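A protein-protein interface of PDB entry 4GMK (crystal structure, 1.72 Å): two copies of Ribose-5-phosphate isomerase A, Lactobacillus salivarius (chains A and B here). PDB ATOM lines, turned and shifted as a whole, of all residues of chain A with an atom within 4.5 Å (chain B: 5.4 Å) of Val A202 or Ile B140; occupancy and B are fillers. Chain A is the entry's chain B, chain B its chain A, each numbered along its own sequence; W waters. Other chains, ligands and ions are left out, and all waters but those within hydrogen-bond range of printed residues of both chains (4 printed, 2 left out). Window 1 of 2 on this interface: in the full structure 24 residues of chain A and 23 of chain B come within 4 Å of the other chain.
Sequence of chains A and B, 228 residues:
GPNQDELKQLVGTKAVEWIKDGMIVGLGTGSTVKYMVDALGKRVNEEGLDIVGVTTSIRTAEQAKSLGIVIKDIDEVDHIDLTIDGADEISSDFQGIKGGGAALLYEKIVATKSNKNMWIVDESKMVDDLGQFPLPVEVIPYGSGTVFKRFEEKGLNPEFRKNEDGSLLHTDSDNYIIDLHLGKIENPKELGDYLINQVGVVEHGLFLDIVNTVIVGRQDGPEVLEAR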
ATOM      1  N   LEU A 105     -36.562  28.159 -18.824  1.00  0.00           N
ATOM      2  CA  LEU A 105     -35.320  27.396 -18.592  1.00  0.00           C
ATOM      3  C   LEU A 105     -35.141  27.097 -17.118  1.00  0.00           C
ATOM      4  O   LEU A 105     -34.983  25.926 -16.738  1.00  0.00           O
ATOM      5  CB  LEU A 105     -34.089  28.113 -19.202  1.00  0.00           C
ATOM      6  CG  LEU A 105     -32.748  27.412 -18.961  1.00  0.00           C
ATOM      7  CD1 LEU A 105     -32.699  25.970 -19.511  1.00  0.00           C
ATOM      8  CD2 LEU A 105     -31.614  28.244 -19.585  1.00  0.00           C
ATOM      9  N   ILE A 109     -35.264  23.451 -15.164  1.00  0.00           N
ATOM     10  CA  ILE A 109     -34.103  22.971 -14.357  1.00  0.00           C
ATOM     11  C   ILE A 109     -34.650  22.544 -12.944  1.00  0.00           C
ATOM     12  O   ILE A 109     -34.335  21.447 -12.462  1.00  0.00           O
ATOM     13  CB  ILE A 109     -33.040  24.067 -14.283  1.00  0.00           C
ATOM     14  CG1 ILE A 109     -32.435  24.201 -15.688  1.00  0.00           C
ATOM     15  CG2 ILE A 109     -32.027  23.731 -13.201  1.00  0.00           C
ATOM     16  CD1 ILE A 109     -31.441  25.373 -15.851  1.00  0.00           C
ATOM     17  N   GLU A 138     -36.163  29.113 -26.097  1.00  0.00           N
ATOM     18  CA  GLU A 138     -35.022  29.946 -25.676  1.00  0.00           C
ATOM     19  C   GLU A 138     -33.855  29.697 -26.643  1.00  0.00           C
ATOM     20  O   GLU A 138     -33.490  28.534 -26.926  1.00  0.00           O
ATOM     21  CB  GLU A 138     -34.643  29.640 -24.213  1.00  0.00           C
ATOM     22  CG  GLU A 138     -33.492  30.571 -23.720  1.00  0.00           C
ATOM     23  CD  GLU A 138     -33.486  30.749 -22.196  1.00  0.00           C
ATOM     24  OE1 GLU A 138     -34.492  30.400 -21.567  1.00  0.00           O
ATOM     25  OE2 GLU A 138     -32.467  31.267 -21.664  1.00  0.00           O
ATOM     26  N   VAL A 139     -33.304  30.784 -27.210  1.00  0.00           N
ATOM     27  CA  VAL A 139     -32.382  30.677 -28.325  1.00  0.00           C
ATOM     28  C   VAL A 139     -31.103  31.491 -28.047  1.00  0.00           C
ATOM     29  O   VAL A 139     -31.193  32.642 -27.584  1.00  0.00           O
ATOM     30  CB  VAL A 139     -33.075  31.197 -29.627  1.00  0.00           C
ATOM     31  CG1 VAL A 139     -32.119  31.185 -30.789  1.00  0.00           C
ATOM     32  CG2 VAL A 139     -34.305  30.344 -29.963  1.00  0.00           C
ATOM     33  N   ILE A 140     -29.916  30.900 -28.337  1.00  0.00           N
ATOM     34  CA  ILE A 140     -28.626  31.660 -28.257  1.00  0.00           C
ATOM     35  C   ILE A 140     -28.675  32.903 -29.212  1.00  0.00           C
ATOM     36  O   ILE A 140     -29.044  32.790 -30.362  1.00  0.00           O
ATOM     37  CB  ILE A 140     -27.476  30.657 -28.675  1.00  0.00           C
ATOM     38  CG1 ILE A 140     -27.372  29.535 -27.629  1.00  0.00           C
ATOM     39  CG2 ILE A 140     -26.138  31.436 -28.944  1.00  0.00           C
ATOM     40  CD1 ILE A 140     -26.863  29.950 -26.237  1.00  0.00           C
ATOM     41  N   SER A 173     -30.592  33.927 -18.443  1.00  0.00           N
ATOM     42  CA  SER A 173     -29.311  33.446 -18.954  1.00  0.00           C
ATOM     43  C   SER A 173     -28.787  34.254 -20.125  1.00  0.00           C
ATOM     44  O   SER A 173     -27.872  33.778 -20.834  1.00  0.00           O
ATOM     45  CB  SER A 173     -29.440  31.970 -19.411  1.00  0.00           C
ATOM     46  OG  SER A 173     -29.669  31.166 -18.266  1.00  0.00           O
ATOM     47  N   ASN A 175     -30.300  34.956 -23.075  1.00  0.00           N
ATOM     48  CA  ASN A 175     -30.721  34.449 -24.410  1.00  0.00           C
ATOM     49  C   ASN A 175     -31.947  35.177 -24.843  1.00  0.00           C
ATOM     50  O   ASN A 175     -32.509  35.984 -24.092  1.00  0.00           O
ATOM     51  CB  ASN A 175     -31.025  32.941 -24.253  1.00  0.00           C
ATOM     52  CG  ASN A 175     -29.788  32.193 -23.876  1.00  0.00           C
ATOM     53  OD1 ASN A 175     -29.765  31.365 -22.914  1.00  0.00           O
ATOM     54  ND2 ASN A 175     -28.739  32.509 -24.574  1.00  0.00           N
ATOM     55  N   ILE A 196     -35.231  20.652 -29.792  1.00  0.00           N
ATOM     56  CA  ILE A 196     -34.028  20.536 -28.953  1.00  0.00           C
ATOM     57  C   ILE A 196     -32.838  20.111 -29.819  1.00  0.00           C
ATOM     58  O   ILE A 196     -31.678  20.404 -29.483  1.00  0.00           O
ATOM     59  CB  ILE A 196     -34.245  19.637 -27.727  1.00  0.00           C
ATOM     60  CG1 ILE A 196     -33.254  20.035 -26.593  1.00  0.00           C
ATOM     61  CG2 ILE A 196     -34.121  18.169 -28.108  1.00  0.00           C
ATOM     62  CD1 ILE A 196     -33.560  21.412 -25.903  1.00  0.00           C
ATOM     63  N   GLY A 200     -28.315  25.898 -31.347  1.00  0.00           N
ATOM     64  CA  GLY A 200     -28.649  27.231 -30.834  1.00  0.00           C
ATOM     65  C   GLY A 200     -29.976  27.261 -30.041  1.00  0.00           C
ATOM     66  O   GLY A 200     -30.251  28.263 -29.335  1.00  0.00           O
ATOM     67  N   VAL A 201     -30.790  26.188 -30.086  1.00  0.00           N
ATOM     68  CA  VAL A 201     -31.972  26.123 -29.186  1.00  0.00           C
ATOM     69  C   VAL A 201     -31.502  25.620 -27.817  1.00  0.00           C
ATOM     70  O   VAL A 201     -30.961  24.525 -27.728  1.00  0.00           O
ATOM     71  CB  VAL A 201     -33.065  25.175 -29.728  1.00  0.00           C
ATOM     72  CG1 VAL A 201     -34.204  24.887 -28.674  1.00  0.00           C
ATOM     73  CG2 VAL A 201     -33.685  25.781 -30.940  1.00  0.00           C
ATOM     74  N   VAL A 202     -31.630  26.441 -26.769  1.00  0.00           N
ATOM     75  CA  VAL A 202     -31.158  26.080 -25.443  1.00  0.00           C
ATOM     76  C   VAL A 202     -32.215  25.155 -24.774  1.00  0.00           C
ATOM     77  O   VAL A 202     -31.886  24.125 -24.157  1.00  0.00           O
ATOM     78  CB  VAL A 202     -30.972  27.387 -24.600  1.00  0.00           C
ATOM     79  CG1 VAL A 202     -30.600  27.000 -23.150  1.00  0.00           C
ATOM     80  CG2 VAL A 202     -29.904  28.265 -25.323  1.00  0.00           C
ATOM     81  N   GLU A 203     -33.491  25.542 -24.905  1.00  0.00           N
ATOM     82  CA  GLU A 203     -34.580  24.789 -24.243  1.00  0.00           C
ATOM     83  C   GLU A 203     -35.887  25.268 -24.834  1.00  0.00           C
ATOM     84  O   GLU A 203     -35.903  26.332 -25.454  1.00  0.00           O
ATOM     85  CB  GLU A 203     -34.516  25.078 -22.717  1.00  0.00           C
ATOM     86  CG  GLU A 203     -35.475  24.194 -21.889  1.00  0.00           C
ATOM     87  CD  GLU A 203     -35.349  22.726 -22.270  1.00  0.00           C
ATOM     88  OE1 GLU A 203     -34.345  22.056 -21.791  1.00  0.00           O
ATOM     89  OE2 GLU A 203     -36.193  22.211 -23.085  1.00  0.00           O
ATOM     90  N   GLU B 138     -21.136  22.183 -23.143  1.00  0.00           N
ATOM     91  CA  GLU B 138     -21.373  23.580 -22.724  1.00  0.00           C
ATOM     92  C   GLU B 138     -22.680  23.573 -21.878  1.00  0.00           C
ATOM     93  O   GLU B 138     -23.696  22.996 -22.314  1.00  0.00           O
ATOM     94  CB  GLU B 138     -21.568  24.523 -23.941  1.00  0.00           C
ATOM     95  CG  GLU B 138     -21.703  25.983 -23.522  1.00  0.00           C
ATOM     96  CD  GLU B 138     -21.123  26.942 -24.560  1.00  0.00           C
ATOM     97  OE1 GLU B 138     -20.415  26.472 -25.470  1.00  0.00           O
ATOM     98  OE2 GLU B 138     -21.442  28.165 -24.503  1.00  0.00           O
ATOM     99  N   VAL B 139     -22.588  24.139 -20.675  1.00  0.00           N
ATOM    100  CA  VAL B 139     -23.711  24.015 -19.698  1.00  0.00           C
ATOM    101  C   VAL B 139     -24.139  25.356 -19.140  1.00  0.00           C
ATOM    102  O   VAL B 139     -23.293  26.229 -18.883  1.00  0.00           O
ATOM    103  CB  VAL B 139     -23.411  23.009 -18.517  1.00  0.00           C
ATOM    104  CG1 VAL B 139     -23.036  21.638 -19.101  1.00  0.00           C
ATOM    105  CG2 VAL B 139     -22.250  23.473 -17.689  1.00  0.00           C
ATOM    106  N   ILE B 140     -25.452  25.495 -18.935  1.00  0.00           N
ATOM    107  CA  ILE B 140     -26.022  26.723 -18.349  1.00  0.00           C
ATOM    108  C   ILE B 140     -25.459  26.813 -16.897  1.00  0.00           C
ATOM    109  O   ILE B 140     -25.478  25.818 -16.162  1.00  0.00           O
ATOM    110  CB  ILE B 140     -27.565  26.592 -18.363  1.00  0.00           C
ATOM    111  CG1 ILE B 140     -28.128  26.640 -19.828  1.00  0.00           C
ATOM    112  CG2 ILE B 140     -28.244  27.607 -17.390  1.00  0.00           C
ATOM    113  CD1 ILE B 140     -27.991  28.010 -20.526  1.00  0.00           C
ATOM    114  N   PRO B 141     -25.029  28.016 -16.449  1.00  0.00           N
ATOM    115  CA  PRO B 141     -24.462  28.130 -15.066  1.00  0.00           C
ATOM    116  C   PRO B 141     -25.437  27.784 -13.928  1.00  0.00           C
ATOM    117  O   PRO B 141     -25.042  27.056 -12.998  1.00  0.00           O
ATOM    118  CB  PRO B 141     -24.058  29.611 -15.006  1.00  0.00           C
ATOM    119  CG  PRO B 141     -23.593  29.847 -16.431  1.00  0.00           C
ATOM    120  CD  PRO B 141     -24.703  29.201 -17.270  1.00  0.00           C
ATOM    121  N   TYR B 142     -26.687  28.282 -14.009  1.00  0.00           N
ATOM    122  CA  TYR B 142     -27.700  27.980 -12.999  1.00  0.00           C
ATOM    123  C   TYR B 142     -27.967  26.474 -13.013  1.00  0.00           C
ATOM    124  O   TYR B 142     -28.339  25.901 -14.099  1.00  0.00           O
ATOM    125  CB  TYR B 142     -28.997  28.727 -13.353  1.00  0.00           C
ATOM    126  CG  TYR B 142     -30.144  28.404 -12.352  1.00  0.00           C
ATOM    127  CD1 TYR B 142     -30.126  28.957 -11.050  1.00  0.00           C
ATOM    128  CD2 TYR B 142     -31.205  27.556 -12.701  1.00  0.00           C
ATOM    129  CE1 TYR B 142     -31.136  28.677 -10.134  1.00  0.00           C
ATOM    130  CE2 TYR B 142     -32.232  27.253 -11.774  1.00  0.00           C
ATOM    131  CZ  TYR B 142     -32.164  27.822 -10.502  1.00  0.00           C
ATOM    132  OH  TYR B 142     -33.144  27.568  -9.576  1.00  0.00           O
ATOM    133  N   GLY B 143     -27.790  25.813 -11.880  1.00  0.00           N
ATOM    134  CA  GLY B 143     -28.042  24.368 -11.884  1.00  0.00           C
ATOM    135  C   GLY B 143     -26.857  23.530 -12.405  1.00  0.00           C
ATOM    136  O   GLY B 143     -26.957  22.313 -12.392  1.00  0.00           O
ATOM    137  N   SER B 144     -25.712  24.138 -12.722  1.00  0.00           N
ATOM    138  CA  SER B 144     -24.614  23.389 -13.309  1.00  0.00           C
ATOM    139  C   SER B 144     -23.915  22.444 -12.329  1.00  0.00           C
ATOM    140  O   SER B 144     -23.332  21.468 -12.753  1.00  0.00           O
ATOM    141  CB  SER B 144     -23.567  24.314 -13.936  1.00  0.00           C
ATOM    142  OG  SER B 144     -23.061  25.194 -12.910  1.00  0.00           O
ATOM    143  N   ASN B 175     -21.466  30.689 -20.744  1.00  0.00           N
ATOM    144  CA  ASN B 175     -21.774  29.415 -20.127  1.00  0.00           C
ATOM    145  C   ASN B 175     -20.491  28.775 -19.543  1.00  0.00           C
ATOM    146  O   ASN B 175     -19.394  29.293 -19.740  1.00  0.00           O
ATOM    147  CB  ASN B 175     -22.380  28.502 -21.233  1.00  0.00           C
ATOM    148  CG  ASN B 175     -23.699  29.027 -21.755  1.00  0.00           C
ATOM    149  OD1 ASN B 175     -23.907  29.111 -22.966  1.00  0.00           O
ATOM    150  ND2 ASN B 175     -24.596  29.375 -20.857  1.00  0.00           N
ATOM    151  N   TYR B 176     -20.603  27.672 -18.821  1.00  0.00           N
ATOM    152  CA  TYR B 176     -19.452  26.916 -18.368  1.00  0.00           C
ATOM    153  C   TYR B 176     -19.258  25.735 -19.345  1.00  0.00           C
ATOM    154  O   TYR B 176     -20.130  25.463 -20.197  1.00  0.00           O
ATOM    155  CB  TYR B 176     -19.666  26.277 -17.002  1.00  0.00           C
ATOM    156  CG  TYR B 176     -19.939  27.316 -15.904  1.00  0.00           C
ATOM    157  CD1 TYR B 176     -19.367  28.565 -15.964  1.00  0.00           C
ATOM    158  CD2 TYR B 176     -20.814  27.028 -14.873  1.00  0.00           C
ATOM    159  CE1 TYR B 176     -19.592  29.505 -14.949  1.00  0.00           C
ATOM    160  CE2 TYR B 176     -21.098  27.960 -13.885  1.00  0.00           C
ATOM    161  CZ  TYR B 176     -20.468  29.182 -13.923  1.00  0.00           C
ATOM    162  OH  TYR B 176     -20.735  30.097 -12.918  1.00  0.00           O
ATOM    163  N   GLY B 200     -30.346  21.938 -19.356  1.00  0.00           N
ATOM    164  CA  GLY B 200     -29.192  22.691 -18.895  1.00  0.00           C
ATOM    165  C   GLY B 200     -27.986  22.483 -19.839  1.00  0.00           C
ATOM    166  O   GLY B 200     -27.030  23.271 -19.776  1.00  0.00           O
ATOM    167  N   VAL B 201     -28.045  21.502 -20.743  1.00  0.00           N
ATOM    168  CA  VAL B 201     -26.917  21.309 -21.693  1.00  0.00           C
ATOM    169  C   VAL B 201     -27.252  22.169 -22.925  1.00  0.00           C
ATOM    170  O   VAL B 201     -28.313  21.993 -23.552  1.00  0.00           O
ATOM    171  CB  VAL B 201     -26.742  19.823 -22.095  1.00  0.00           C
ATOM    172  CG1 VAL B 201     -25.758  19.753 -23.285  1.00  0.00           C
ATOM    173  CG2 VAL B 201     -26.143  19.005 -20.917  1.00  0.00           C
ATOM    174  N   VAL B 202     -26.380  23.125 -23.238  1.00  0.00           N
ATOM    175  CA  VAL B 202     -26.573  24.019 -24.394  1.00  0.00           C
ATOM    176  C   VAL B 202     -26.144  23.315 -25.686  1.00  0.00           C
ATOM    177  O   VAL B 202     -26.884  23.345 -26.663  1.00  0.00           O
ATOM    178  CB  VAL B 202     -25.695  25.258 -24.218  1.00  0.00           C
ATOM    179  CG1 VAL B 202     -25.916  26.204 -25.402  1.00  0.00           C
ATOM    180  CG2 VAL B 202     -26.109  25.984 -22.916  1.00  0.00           C
HETATM  181  O   HOH W   1     -27.413  23.985 -29.319  1.00  0.00           O
HETATM  182  O   HOH W   2     -31.658  22.664 -21.793  1.00  0.00           O
HETATM  183  O   HOH W   3     -26.748  30.781 -22.392  1.00  0.00           O
HETATM  184  O   HOH W   4     -27.716  30.823 -15.801  1.00  0.00           O
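The backbone carbonyl oxygen (O) of Gly A200 lies within hydrogen-bond range of the backbone NH (N) of Ile A140 (2.8 Å).
The backbone NH (N) of Ile B140 is in hydrogen-bond range of the backbone carbonyl oxygen (O) of Gly B200 (2.9 Å).
O of Glu A138 sits at hydrogen-bond distance from N of Val A202 (2.8 Å).
The backbone NH of Val B202 is in hydrogen-bond range of the backbone carbonyl oxygen of Glu B138 (2.8 Å).
Among the printed residues, merely in contact across the chains: Leu A105 with Ile B140 (3.8 Å), Ile A109 with Tyr B142 (3.6 Å), Ile A140 with Val B202 (3.95 Å), Ser A173 with Ile B140 (3.9 Å) and Val A202 with Ile B140 (3.8 Å).
Of the printed residues of chain B, Leu A105 touches Ile B140.
Of the printed residues of chain B, Ile A140 touches Val B202.
Ile B140 touches just these residues of chain A: Leu A105 (3.8 Å), Ser A173 (3.9 Å) and Val A202 (3.8 Å).
Of the printed residues of chain A, Tyr B142 touches Ile A109.
Of the printed residues of chain A, Val B202 touches Ile A140 (3.95 Å).
The nearest printed residue of chain B that does not touch Ser A173 is Pro B141 (5.4 Å).
Hydrophobic or aromatic side chains of chain B that line the printed part of chain A: Ile B140, Tyr B142 and Val B202.
Of the 12 printed residues of chain A, 5 touch a printed residue of chain B.
Hydrophobic or aromatic side chains of chain A that line the printed part of chain B: Leu A105, Ile A109, Ile A140 and Val A202.
Ile A140 touches Val B202, and with the chains exchanged Val A202 touches Ile B140.
Water W2 lies within hydrogen-bond range of OE1 of Glu A203 (2.8 Å), O of Val A202 (2.8 Å) and N of Gly B200 (2.9 Å).
Water W1 bridges the backbone carbonyl oxygen of Val B202 and the backbone NH of Gly A200.
Water W3 lies within hydrogen-bond range of the side-chain amide nitrogen (ND2) of Asn B175 (3.0 Å) and the side-chain amide oxygen (OD1) of Asn A175 (3.1 Å).
Water W4 lies within hydrogen-bond range of OG of Ser A173 and N of Tyr B142.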
